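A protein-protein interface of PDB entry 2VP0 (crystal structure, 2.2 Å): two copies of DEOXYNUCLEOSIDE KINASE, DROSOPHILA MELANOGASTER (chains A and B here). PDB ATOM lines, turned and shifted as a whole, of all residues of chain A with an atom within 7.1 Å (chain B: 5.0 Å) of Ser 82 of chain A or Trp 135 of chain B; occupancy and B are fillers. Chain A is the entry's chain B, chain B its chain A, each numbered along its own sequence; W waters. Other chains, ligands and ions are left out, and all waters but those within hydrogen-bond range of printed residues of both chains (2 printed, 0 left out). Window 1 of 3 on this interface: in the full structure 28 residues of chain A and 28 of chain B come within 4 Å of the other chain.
OG of Ser 82 of chain B is in hydrogen-bond range of NE1 of Trp 135 of chain A, at 3.0 Å.
NE1 of Trp 135 of chain B sits at hydrogen-bond distance from OG of Ser 82 of chain A, at 2.8 Å.
O of Tyr 83 of chain A lies within hydrogen-bond range of OG1 of Thr 87 of chain A (3.5 Å).
Among the printed residues, merely in contact across the chains: Leu 86 of chain A with Glu 134 of chain B (3.4 Å), Leu 86 of chain A with Trp 135 of chain B (3.4 Å), Leu 65 of chain A with Thr 131 of chain B (3.5 Å), Leu 86 of chain A with Phe 138 of chain B (3.5 Å), Pro 79 of chain A with Thr 131 of chain B (3.6 Å), Ile 143 of chain A with Phe 138 of chain B (3.7 Å), Tyr 83 of chain A with Glu 134 of chain B (3.7 Å), Trp 135 of chain A with Trp 135 of chain B (3.8 Å), Ser 82 of chain A with Thr 131 of chain B (3.9 Å), Leu 89 of chain A with Trp 135 of chain B (3.9 Å), Tyr 83 of chain A with Thr 131 of chain B (3.98 Å) and Trp 135 of chain A with Ile 139 of chain B (3.999 Å).
Ser 82 of chain A touches just these residues of chain B: Thr 131 and Trp 135.
Of chain A, only Ser 82 (2.8 Å), Leu 86 (3.4 Å), Leu 89 (3.9 Å) and Trp 135 (3.8 Å) come within 4 Å of Trp 135 of chain B.
Printed residues of chain B within 4 Å of Pro 79 of chain A: Thr 131.
Printed residues of chain B within 4 Å of Leu 65 of chain A: Thr 131.
The nearest residue of chain B that does not touch Ser 82 of chain A is Ser 82 of chain B (4.6 Å).
The nearest printed residue of chain A that does not touch Ile 139 of chain B is Leu 86 of chain A (6.1 Å).
Hydrophobic or aromatic side chains of chain B within 4 Å of the printed part of chain A: Trp 135, Phe 138 and Ile 139.
Among the printed residues, 14 pairs touch across the chains.
Among the printed residues, no Asp or Glu carboxylate lies within 4 Å of a Lys or Arg side-chain nitrogen of the other chain.
Ser 82 of chain A touches Trp 135 of chain B, and with the chains exchanged Trp 135 of chain A touches Ser 82 of chain B.
Trp 135 of chain B touches its own counterpart, Trp 135 of chain A.
Trp 135 of chain A touches Ile 139 of chain B, but with the chains exchanged Ile 139 of chain A does not touch Trp 135 of chain B (4.2 Å).
Of the 14 pairs that touch across the chains among the printed residues, 3 have their exchanged pair printed and touching as well.
Water W2 bridges OG of Ser 82 of chain A and OG of Ser 82 of chain B.
Water W1 lies within hydrogen-bond range of O of Glu 134 of chain B (2.9 Å) and NE2 of Gln 90 of chain A (3.1 Å).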
ATOM      1  N   LEU A  65      -0.070  -7.073 -24.389  1.00  0.00           N
ATOM      2  CA  LEU A  65       0.415  -8.439 -24.164  1.00  0.00           C
ATOM      3  C   LEU A  65      -0.695  -9.490 -24.283  1.00  0.00           C
ATOM      4  O   LEU A  65      -0.434 -10.627 -24.676  1.00  0.00           O
ATOM      5  CB  LEU A  65       1.102  -8.565 -22.793  1.00  0.00           C
ATOM      6  CG  LEU A  65       2.458  -7.890 -22.538  1.00  0.00           C
ATOM      7  CD1 LEU A  65       2.966  -8.250 -21.146  1.00  0.00           C
ATOM      8  CD2 LEU A  65       3.508  -8.268 -23.610  1.00  0.00           C
ATOM      9  N   TRP A  76       4.497 -15.754 -26.961  1.00  0.00           N
ATOM     10  CA  TRP A  76       4.081 -14.703 -26.029  1.00  0.00           C
ATOM     11  C   TRP A  76       3.386 -15.137 -24.736  1.00  0.00           C
ATOM     12  O   TRP A  76       3.209 -14.311 -23.830  1.00  0.00           O
ATOM     13  CB  TRP A  76       3.225 -13.664 -26.754  1.00  0.00           C
ATOM     14  CG  TRP A  76       4.024 -12.809 -27.665  1.00  0.00           C
ATOM     15  CD1 TRP A  76       4.223 -12.990 -29.004  1.00  0.00           C
ATOM     16  CD2 TRP A  76       4.766 -11.639 -27.300  1.00  0.00           C
ATOM     17  NE1 TRP A  76       5.035 -11.992 -29.503  1.00  0.00           N
ATOM     18  CE2 TRP A  76       5.383 -11.151 -28.478  1.00  0.00           C
ATOM     19  CE3 TRP A  76       4.958 -10.951 -26.098  1.00  0.00           C
ATOM     20  CZ2 TRP A  76       6.182  -9.995 -28.484  1.00  0.00           C
ATOM     21  CZ3 TRP A  76       5.761  -9.802 -26.098  1.00  0.00           C
ATOM     22  CH2 TRP A  76       6.359  -9.339 -27.285  1.00  0.00           C
ATOM     23  N   ALA A  77       3.006 -16.419 -24.633  1.00  0.00           N
ATOM     24  CA  ALA A  77       2.355 -16.908 -23.416  1.00  0.00           C
ATOM     25  C   ALA A  77       3.261 -16.706 -22.207  1.00  0.00           C
ATOM     26  O   ALA A  77       2.806 -16.326 -21.123  1.00  0.00           O
ATOM     27  CB  ALA A  77       1.950 -18.374 -23.549  1.00  0.00           C
ATOM     28  N   MET A  78       4.548 -16.946 -22.409  1.00  0.00           N
ATOM     29  CA  MET A  78       5.545 -16.839 -21.340  1.00  0.00           C
ATOM     30  C   MET A  78       5.703 -15.424 -20.787  1.00  0.00           C
ATOM     31  O   MET A  78       5.535 -15.204 -19.577  1.00  0.00           O
ATOM     32  CB  MET A  78       6.885 -17.342 -21.852  1.00  0.00           C
ATOM     33  CG  MET A  78       7.496 -18.382 -20.995  1.00  0.00           C
ATOM     34  SD  MET A  78       8.036 -17.912 -19.374  1.00  0.00           S
ATOM     35  CE  MET A  78       8.749 -16.290 -19.716  1.00  0.00           C
ATOM     36  N   PRO A  79       6.056 -14.460 -21.656  1.00  0.00           N
ATOM     37  CA  PRO A  79       6.097 -13.082 -21.162  1.00  0.00           C
ATOM     38  C   PRO A  79       4.749 -12.609 -20.592  1.00  0.00           C
ATOM     39  O   PRO A  79       4.736 -11.895 -19.588  1.00  0.00           O
ATOM     40  CB  PRO A  79       6.501 -12.257 -22.401  1.00  0.00           C
ATOM     41  CG  PRO A  79       6.282 -13.156 -23.577  1.00  0.00           C
ATOM     42  CD  PRO A  79       6.470 -14.556 -23.066  1.00  0.00           C
ATOM     43  N   PHE A  80       3.634 -13.029 -21.202  1.00  0.00           N
ATOM     44  CA  PHE A  80       2.310 -12.582 -20.737  1.00  0.00           C
ATOM     45  C   PHE A  80       2.023 -13.072 -19.315  1.00  0.00           C
ATOM     46  O   PHE A  80       1.658 -12.278 -18.447  1.00  0.00           O
ATOM     47  CB  PHE A  80       1.193 -13.010 -21.708  1.00  0.00           C
ATOM     48  CG  PHE A  80      -0.190 -12.832 -21.153  1.00  0.00           C
ATOM     49  CD1 PHE A  80      -0.816 -11.593 -21.199  1.00  0.00           C
ATOM     50  CD2 PHE A  80      -0.856 -13.911 -20.562  1.00  0.00           C
ATOM     51  CE1 PHE A  80      -2.092 -11.420 -20.668  1.00  0.00           C
ATOM     52  CE2 PHE A  80      -2.127 -13.759 -20.044  1.00  0.00           C
ATOM     53  CZ  PHE A  80      -2.756 -12.522 -20.093  1.00  0.00           C
ATOM     54  N   GLN A  81       2.221 -14.367 -19.071  1.00  0.00           N
ATOM     55  CA  GLN A  81       2.037 -14.939 -17.728  1.00  0.00           C
ATOM     56  C   GLN A  81       3.013 -14.393 -16.668  1.00  0.00           C
ATOM     57  O   GLN A  81       2.651 -14.208 -15.499  1.00  0.00           O
ATOM     58  CB  GLN A  81       2.122 -16.468 -17.773  1.00  0.00           C
ATOM     59  CG  GLN A  81       0.918 -17.160 -18.414  1.00  0.00           C
ATOM     60  CD  GLN A  81      -0.447 -16.711 -17.864  1.00  0.00           C
ATOM     61  OE1 GLN A  81      -1.394 -16.568 -18.628  1.00  0.00           O
ATOM     62  NE2 GLN A  81      -0.548 -16.507 -16.554  1.00  0.00           N
ATOM     63  N   SER A  82       4.252 -14.139 -17.076  1.00  0.00           N
ATOM     64  CA  SER A  82       5.223 -13.529 -16.184  1.00  0.00           C
ATOM     65  C   SER A  82       4.739 -12.142 -15.763  1.00  0.00           C
ATOM     66  O   SER A  82       4.874 -11.753 -14.594  1.00  0.00           O
ATOM     67  CB  SER A  82       6.587 -13.429 -16.879  1.00  0.00           C
ATOM     68  OG  SER A  82       7.494 -12.699 -16.078  1.00  0.00           O
ATOM     69  N   TYR A  83       4.177 -11.393 -16.709  1.00  0.00           N
ATOM     70  CA  TYR A  83       3.644 -10.071 -16.382  1.00  0.00           C
ATOM     71  C   TYR A  83       2.358 -10.161 -15.529  1.00  0.00           C
ATOM     72  O   TYR A  83       2.154  -9.342 -14.635  1.00  0.00           O
ATOM     73  CB  TYR A  83       3.419  -9.228 -17.646  1.00  0.00           C
ATOM     74  CG  TYR A  83       3.060  -7.801 -17.342  1.00  0.00           C
ATOM     75  CD1 TYR A  83       4.017  -6.912 -16.853  1.00  0.00           C
ATOM     76  CD2 TYR A  83       1.758  -7.336 -17.521  1.00  0.00           C
ATOM     77  CE1 TYR A  83       3.679  -5.588 -16.542  1.00  0.00           C
ATOM     78  CE2 TYR A  83       1.412  -6.021 -17.218  1.00  0.00           C
ATOM     79  CZ  TYR A  83       2.370  -5.146 -16.735  1.00  0.00           C
ATOM     80  OH  TYR A  83       2.024  -3.834 -16.445  1.00  0.00           O
ATOM     81  N   VAL A  84       1.503 -11.154 -15.796  1.00  0.00           N
ATOM     82  CA  VAL A  84       0.337 -11.376 -14.923  1.00  0.00           C
ATOM     83  C   VAL A  84       0.818 -11.607 -13.510  1.00  0.00           C
ATOM     84  O   VAL A  84       0.301 -11.006 -12.557  1.00  0.00           O
ATOM     85  CB  VAL A  84      -0.594 -12.571 -15.362  1.00  0.00           C
ATOM     86  CG1 VAL A  84      -1.682 -12.828 -14.303  1.00  0.00           C
ATOM     87  CG2 VAL A  84      -1.241 -12.279 -16.701  1.00  0.00           C
ATOM     88  N   THR A  85       1.816 -12.481 -13.379  1.00  0.00           N
ATOM     89  CA  THR A  85       2.365 -12.809 -12.072  1.00  0.00           C
ATOM     90  C   THR A  85       2.803 -11.552 -11.333  1.00  0.00           C
ATOM     91  O   THR A  85       2.425 -11.345 -10.186  1.00  0.00           O
ATOM     92  CB  THR A  85       3.498 -13.838 -12.175  1.00  0.00           C
ATOM     93  OG1 THR A  85       2.948 -15.073 -12.654  1.00  0.00           O
ATOM     94  CG2 THR A  85       4.123 -14.088 -10.799  1.00  0.00           C
ATOM     95  N   LEU A  86       3.573 -10.704 -12.010  1.00  0.00           N
ATOM     96  CA  LEU A  86       4.002  -9.426 -11.462  1.00  0.00           C
ATOM     97  C   LEU A  86       2.848  -8.528 -10.992  1.00  0.00           C
ATOM     98  O   LEU A  86       2.898  -8.005  -9.883  1.00  0.00           O
ATOM     99  CB  LEU A  86       4.856  -8.662 -12.484  1.00  0.00           C
ATOM    100  CG  LEU A  86       5.341  -7.261 -12.079  1.00  0.00           C
ATOM    101  CD1 LEU A  86       6.022  -7.266 -10.710  1.00  0.00           C
ATOM    102  CD2 LEU A  86       6.269  -6.698 -13.131  1.00  0.00           C
ATOM    103  N   THR A  87       1.837  -8.319 -11.837  1.00  0.00           N
ATOM    104  CA  THR A  87       0.767  -7.372 -11.493  1.00  0.00           C
ATOM    105  C   THR A  87      -0.068  -7.859 -10.300  1.00  0.00           C
ATOM    106  O   THR A  87      -0.481  -7.053  -9.475  1.00  0.00           O
ATOM    107  CB  THR A  87      -0.149  -7.001 -12.701  1.00  0.00           C
ATOM    108  OG1 THR A  87      -0.775  -8.177 -13.226  1.00  0.00           O
ATOM    109  CG2 THR A  87       0.653  -6.311 -13.787  1.00  0.00           C
ATOM    110  N   LEU A  89       1.206  -9.792  -7.890  1.00  0.00           N
ATOM    111  CA  LEU A  89       2.128  -9.503  -6.789  1.00  0.00           C
ATOM    112  C   LEU A  89       2.052  -8.058  -6.330  1.00  0.00           C
ATOM    113  O   LEU A  89       2.025  -7.785  -5.123  1.00  0.00           O
ATOM    114  CB  LEU A  89       3.561  -9.846  -7.179  1.00  0.00           C
ATOM    115  CG  LEU A  89       4.225 -10.978  -6.404  1.00  0.00           C
ATOM    116  CD1 LEU A  89       3.232 -12.021  -5.944  1.00  0.00           C
ATOM    117  CD2 LEU A  89       5.310 -11.586  -7.273  1.00  0.00           C
ATOM    118  N   GLN A  90       2.005  -7.142  -7.293  1.00  0.00           N
ATOM    119  CA  GLN A  90       1.875  -5.721  -6.998  1.00  0.00           C
ATOM    120  C   GLN A  90       0.598  -5.451  -6.194  1.00  0.00           C
ATOM    121  O   GLN A  90       0.618  -4.670  -5.238  1.00  0.00           O
ATOM    122  CB  GLN A  90       1.880  -4.884  -8.286  1.00  0.00           C
ATOM    123  CG  GLN A  90       3.199  -4.934  -9.055  1.00  0.00           C
ATOM    124  CD  GLN A  90       3.156  -4.172 -10.371  1.00  0.00           C
ATOM    125  OE1 GLN A  90       2.157  -4.188 -11.100  1.00  0.00           O
ATOM    126  NE2 GLN A  90       4.244  -3.496 -10.680  1.00  0.00           N
ATOM    127  N   ILE A 107      -2.402 -14.416  -7.580  1.00  0.00           N
ATOM    128  CA  ILE A 107      -1.261 -15.163  -8.115  1.00  0.00           C
ATOM    129  C   ILE A 107      -1.581 -16.662  -8.248  1.00  0.00           C
ATOM    130  O   ILE A 107      -1.000 -17.361  -9.090  1.00  0.00           O
ATOM    131  CB  ILE A 107       0.028 -14.939  -7.264  1.00  0.00           C
ATOM    132  CG1 ILE A 107       1.282 -15.356  -8.043  1.00  0.00           C
ATOM    133  CG2 ILE A 107      -0.074 -15.596  -5.871  1.00  0.00           C
ATOM    134  CD1 ILE A 107       2.592 -14.929  -7.386  1.00  0.00           C
ATOM    135  N   VAL A 115      -1.402 -20.957 -16.157  1.00  0.00           N
ATOM    136  CA  VAL A 115      -0.064 -21.485 -16.440  1.00  0.00           C
ATOM    137  C   VAL A 115      -0.118 -23.000 -16.639  1.00  0.00           C
ATOM    138  O   VAL A 115       0.444 -23.524 -17.610  1.00  0.00           O
ATOM    139  CB  VAL A 115       0.987 -21.062 -15.354  1.00  0.00           C
ATOM    140  CG1 VAL A 115       2.262 -21.876 -15.467  1.00  0.00           C
ATOM    141  CG2 VAL A 115       1.306 -19.573 -15.487  1.00  0.00           C
ATOM    142  N   LEU A 132       8.724 -20.140 -14.971  1.00  0.00           N
ATOM    143  CA  LEU A 132       7.580 -19.592 -14.225  1.00  0.00           C
ATOM    144  C   LEU A 132       7.409 -20.269 -12.879  1.00  0.00           C
ATOM    145  O   LEU A 132       7.164 -19.597 -11.876  1.00  0.00           O
ATOM    146  CB  LEU A 132       6.288 -19.664 -15.037  1.00  0.00           C
ATOM    147  CG  LEU A 132       6.198 -18.754 -16.261  1.00  0.00           C
ATOM    148  CD1 LEU A 132       5.077 -19.245 -17.172  1.00  0.00           C
ATOM    149  CD2 LEU A 132       6.013 -17.269 -15.907  1.00  0.00           C
ATOM    150  N   TRP A 135      10.032 -19.209 -10.349  1.00  0.00           N
ATOM    151  CA  TRP A 135       9.625 -17.892  -9.846  1.00  0.00           C
ATOM    152  C   TRP A 135       8.563 -17.986  -8.741  1.00  0.00           C
ATOM    153  O   TRP A 135       8.694 -17.349  -7.691  1.00  0.00           O
ATOM    154  CB  TRP A 135       9.146 -17.001 -10.976  1.00  0.00           C
ATOM    155  CG  TRP A 135      10.204 -16.073 -11.504  1.00  0.00           C
ATOM    156  CD1 TRP A 135      10.841 -16.150 -12.714  1.00  0.00           C
ATOM    157  CD2 TRP A 135      10.743 -14.923 -10.840  1.00  0.00           C
ATOM    158  NE1 TRP A 135      11.733 -15.114 -12.846  1.00  0.00           N
ATOM    159  CE2 TRP A 135      11.697 -14.346 -11.712  1.00  0.00           C
ATOM    160  CE3 TRP A 135      10.516 -14.327  -9.591  1.00  0.00           C
ATOM    161  CZ2 TRP A 135      12.425 -13.193 -11.378  1.00  0.00           C
ATOM    162  CZ3 TRP A 135      11.251 -13.182  -9.252  1.00  0.00           C
ATOM    163  CH2 TRP A 135      12.186 -12.626 -10.150  1.00  0.00           C
ATOM    164  N   TYR A 136       7.541 -18.820  -8.965  1.00  0.00           N
ATOM    165  CA  TYR A 136       6.489 -19.050  -7.965  1.00  0.00           C
ATOM    166  C   TYR A 136       7.035 -19.547  -6.643  1.00  0.00           C
ATOM    167  O   TYR A 136       6.553 -19.153  -5.589  1.00  0.00           O
ATOM    168  CB  TYR A 136       5.400 -20.001  -8.490  1.00  0.00           C
ATOM    169  CG  TYR A 136       4.518 -19.371  -9.542  1.00  0.00           C
ATOM    170  CD1 TYR A 136       4.288 -20.015 -10.760  1.00  0.00           C
ATOM    171  CD2 TYR A 136       3.937 -18.114  -9.335  1.00  0.00           C
ATOM    172  CE1 TYR A 136       3.491 -19.443 -11.734  1.00  0.00           C
ATOM    173  CE2 TYR A 136       3.143 -17.524 -10.320  1.00  0.00           C
ATOM    174  CZ  TYR A 136       2.925 -18.197 -11.510  1.00  0.00           C
ATOM    175  OH  TYR A 136       2.141 -17.638 -12.492  1.00  0.00           O
ATOM    176  N   ILE A 139       8.954 -16.627  -4.933  1.00  0.00           N
ATOM    177  CA  ILE A 139       7.950 -15.664  -4.472  1.00  0.00           C
ATOM    178  C   ILE A 139       7.331 -16.105  -3.132  1.00  0.00           C
ATOM    179  O   ILE A 139       7.171 -15.305  -2.217  1.00  0.00           O
ATOM    180  CB  ILE A 139       6.844 -15.449  -5.559  1.00  0.00           C
ATOM    181  CG1 ILE A 139       7.422 -14.714  -6.776  1.00  0.00           C
ATOM    182  CG2 ILE A 139       5.604 -14.728  -4.980  1.00  0.00           C
ATOM    183  CD1 ILE A 139       6.576 -14.821  -8.035  1.00  0.00           C
ATOM    184  N   ILE A 143       8.036 -13.222  -0.585  1.00  0.00           N
ATOM    185  CA  ILE A 143       6.981 -12.216  -0.636  1.00  0.00           C
ATOM    186  C   ILE A 143       5.720 -12.745   0.049  1.00  0.00           C
ATOM    187  O   ILE A 143       5.275 -13.855  -0.238  1.00  0.00           O
ATOM    188  CB  ILE A 143       6.687 -11.789  -2.097  1.00  0.00           C
ATOM    189  CG1 ILE A 143       7.915 -11.091  -2.705  1.00  0.00           C
ATOM    190  CG2 ILE A 143       5.444 -10.901  -2.174  1.00  0.00           C
ATOM    191  CD1 ILE A 143       7.740 -10.669  -4.128  1.00  0.00           C
ATOM    192  N   SER B  82      14.666 -13.933 -17.779  1.00  0.00           N
ATOM    193  CA  SER B  82      13.834 -14.041 -16.573  1.00  0.00           C
ATOM    194  C   SER B  82      14.428 -15.016 -15.536  1.00  0.00           C
ATOM    195  O   SER B  82      14.460 -14.719 -14.334  1.00  0.00           O
ATOM    196  CB  SER B  82      12.403 -14.468 -16.950  1.00  0.00           C
ATOM    197  OG  SER B  82      11.615 -14.604 -15.775  1.00  0.00           O
ATOM    198  N   THR B 131       8.275  -6.266 -20.072  1.00  0.00           N
ATOM    199  CA  THR B 131       7.956  -7.198 -18.992  1.00  0.00           C
ATOM    200  C   THR B 131       9.128  -7.327 -18.019  1.00  0.00           C
ATOM    201  O   THR B 131       8.959  -7.163 -16.811  1.00  0.00           O
ATOM    202  CB  THR B 131       7.537  -8.568 -19.563  1.00  0.00           C
ATOM    203  OG1 THR B 131       6.306  -8.396 -20.262  1.00  0.00           O
ATOM    204  CG2 THR B 131       7.342  -9.618 -18.443  1.00  0.00           C
ATOM    205  N   LEU B 132      10.317  -7.572 -18.567  1.00  0.00           N
ATOM    206  CA  LEU B 132      11.550  -7.679 -17.786  1.00  0.00           C
ATOM    207  C   LEU B 132      11.846  -6.402 -17.009  1.00  0.00           C
ATOM    208  O   LEU B 132      12.275  -6.468 -15.862  1.00  0.00           O
ATOM    209  CB  LEU B 132      12.738  -8.058 -18.696  1.00  0.00           C
ATOM    210  CG  LEU B 132      12.701  -9.440 -19.363  1.00  0.00           C
ATOM    211  CD1 LEU B 132      13.669  -9.536 -20.571  1.00  0.00           C
ATOM    212  CD2 LEU B 132      12.947 -10.601 -18.400  1.00  0.00           C
ATOM    213  N   GLU B 133      11.591  -5.241 -17.619  1.00  0.00           N
ATOM    214  CA  GLU B 133      11.849  -3.953 -16.965  1.00  0.00           C
ATOM    215  C   GLU B 133      10.880  -3.675 -15.821  1.00  0.00           C
ATOM    216  O   GLU B 133      11.273  -3.142 -14.775  1.00  0.00           O
ATOM    217  CB  GLU B 133      11.817  -2.807 -17.979  1.00  0.00           C
ATOM    218  CG  GLU B 133      13.152  -2.562 -18.653  1.00  0.00           C
ATOM    219  CD  GLU B 133      14.221  -2.078 -17.676  1.00  0.00           C
ATOM    220  OE1 GLU B 133      13.941  -1.149 -16.877  1.00  0.00           O
ATOM    221  OE2 GLU B 133      15.335  -2.632 -17.709  1.00  0.00           O
ATOM    222  N   GLU B 134       9.614  -4.057 -16.021  1.00  0.00           N
ATOM    223  CA  GLU B 134       8.598  -3.935 -14.973  1.00  0.00           C
ATOM    224  C   GLU B 134       8.967  -4.802 -13.782  1.00  0.00           C
ATOM    225  O   GLU B 134       8.818  -4.375 -12.653  1.00  0.00           O
ATOM    226  CB  GLU B 134       7.207  -4.297 -15.507  1.00  0.00           C
ATOM    227  CG  GLU B 134       6.714  -3.395 -16.640  1.00  0.00           C
ATOM    228  CD  GLU B 134       5.717  -2.356 -16.195  1.00  0.00           C
ATOM    229  OE1 GLU B 134       5.156  -1.669 -17.087  1.00  0.00           O
ATOM    230  OE2 GLU B 134       5.477  -2.226 -14.972  1.00  0.00           O
ATOM    231  N   TRP B 135       9.449  -6.013 -14.048  1.00  0.00           N
ATOM    232  CA  TRP B 135      10.020  -6.880 -13.008  1.00  0.00           C
ATOM    233  C   TRP B 135      11.191  -6.216 -12.278  1.00  0.00           C
ATOM    234  O   TRP B 135      11.212  -6.194 -11.047  1.00  0.00           O
ATOM    235  CB  TRP B 135      10.457  -8.226 -13.591  1.00  0.00           C
ATOM    236  CG  TRP B 135       9.397  -9.287 -13.498  1.00  0.00           C
ATOM    237  CD1 TRP B 135       8.688  -9.841 -14.530  1.00  0.00           C
ATOM    238  CD2 TRP B 135       8.919  -9.917 -12.303  1.00  0.00           C
ATOM    239  NE1 TRP B 135       7.804 -10.785 -14.053  1.00  0.00           N
ATOM    240  CE2 TRP B 135       7.917 -10.845 -12.689  1.00  0.00           C
ATOM    241  CE3 TRP B 135       9.243  -9.795 -10.941  1.00  0.00           C
ATOM    242  CZ2 TRP B 135       7.242 -11.644 -11.764  1.00  0.00           C
ATOM    243  CZ3 TRP B 135       8.568 -10.596 -10.021  1.00  0.00           C
ATOM    244  CH2 TRP B 135       7.573 -11.499 -10.434  1.00  0.00           C
ATOM    245  N   TYR B 136      12.142  -5.659 -13.036  1.00  0.00           N
ATOM    246  CA  TYR B 136      13.335  -5.047 -12.453  1.00  0.00           C
ATOM    247  C   TYR B 136      12.950  -3.917 -11.509  1.00  0.00           C
ATOM    248  O   TYR B 136      13.571  -3.739 -10.458  1.00  0.00           O
ATOM    249  CB  TYR B 136      14.301  -4.530 -13.532  1.00  0.00           C
ATOM    250  CG  TYR B 136      15.067  -5.615 -14.241  1.00  0.00           C
ATOM    251  CD1 TYR B 136      15.098  -5.691 -15.639  1.00  0.00           C
ATOM    252  CD2 TYR B 136      15.756  -6.587 -13.508  1.00  0.00           C
ATOM    253  CE1 TYR B 136      15.788  -6.714 -16.277  1.00  0.00           C
ATOM    254  CE2 TYR B 136      16.445  -7.579 -14.129  1.00  0.00           C
ATOM    255  CZ  TYR B 136      16.458  -7.645 -15.507  1.00  0.00           C
ATOM    256  OH  TYR B 136      17.164  -8.657 -16.076  1.00  0.00           O
ATOM    257  N   LYS B 137      11.918  -3.165 -11.901  1.00  0.00           N
ATOM    258  CA  LYS B 137      11.413  -2.047 -11.122  1.00  0.00           C
ATOM    259  C   LYS B 137      10.843  -2.544  -9.803  1.00  0.00           C
ATOM    260  O   LYS B 137      11.184  -2.017  -8.737  1.00  0.00           O
ATOM    261  CB  LYS B 137      10.353  -1.253 -11.923  1.00  0.00           C
ATOM    262  CG  LYS B 137      10.899  -0.577 -13.185  1.00  0.00           C
ATOM    263  CD  LYS B 137       9.830  -0.398 -14.301  1.00  0.00           C
ATOM    264  CE  LYS B 137      10.502  -0.129 -15.677  1.00  0.00           C
ATOM    265  NZ  LYS B 137       9.515   0.001 -16.827  1.00  0.00           N
ATOM    266  N   PHE B 138       9.991  -3.571  -9.877  1.00  0.00           N
ATOM    267  CA  PHE B 138       9.377  -4.143  -8.675  1.00  0.00           C
ATOM    268  C   PHE B 138      10.392  -4.793  -7.730  1.00  0.00           C
ATOM    269  O   PHE B 138      10.270  -4.678  -6.506  1.00  0.00           O
ATOM    270  CB  PHE B 138       8.270  -5.145  -9.050  1.00  0.00           C
ATOM    271  CG  PHE B 138       7.651  -5.846  -7.870  1.00  0.00           C
ATOM    272  CD1 PHE B 138       6.720  -5.197  -7.067  1.00  0.00           C
ATOM    273  CD2 PHE B 138       7.983  -7.161  -7.574  1.00  0.00           C
ATOM    274  CE1 PHE B 138       6.133  -5.845  -5.981  1.00  0.00           C
ATOM    275  CE2 PHE B 138       7.404  -7.809  -6.489  1.00  0.00           C
ATOM    276  CZ  PHE B 138       6.480  -7.146  -5.693  1.00  0.00           C
ATOM    277  N   ILE B 139      11.368  -5.497  -8.303  1.00  0.00           N
ATOM    278  CA  ILE B 139      12.446  -6.122  -7.537  1.00  0.00           C
ATOM    279  C   ILE B 139      13.196  -5.071  -6.721  1.00  0.00           C
ATOM    280  O   ILE B 139      13.526  -5.294  -5.551  1.00  0.00           O
ATOM    281  CB  ILE B 139      13.420  -6.925  -8.471  1.00  0.00           C
ATOM    282  CG1 ILE B 139      12.750  -8.224  -8.949  1.00  0.00           C
ATOM    283  CG2 ILE B 139      14.750  -7.234  -7.758  1.00  0.00           C
ATOM    284  CD1 ILE B 139      13.348  -8.800 -10.206  1.00  0.00           C
ATOM    285  N   GLU B 140      13.437  -3.919  -7.338  1.00  0.00           N
ATOM    286  CA  GLU B 140      14.107  -2.817  -6.667  1.00  0.00           C
ATOM    287  C   GLU B 140      13.314  -2.312  -5.445  1.00  0.00           C
ATOM    288  O   GLU B 140      13.903  -1.931  -4.436  1.00  0.00           O
ATOM    289  CB  GLU B 140      14.376  -1.684  -7.656  1.00  0.00           C
ATOM    290  CG  GLU B 140      15.468  -0.718  -7.211  1.00  0.00           C
ATOM    291  CD  GLU B 140      15.765   0.323  -8.254  1.00  0.00           C
ATOM    292  OE1 GLU B 140      15.233   1.448  -8.122  1.00  0.00           O
ATOM    293  OE2 GLU B 140      16.519   0.019  -9.206  1.00  0.00           O
HETATM  294  O   HOH W   1       6.857  -2.371 -11.855  1.00  0.00           O
HETATM  295  O   HOH W   2       8.935 -14.788 -15.355  1.00  0.00           O
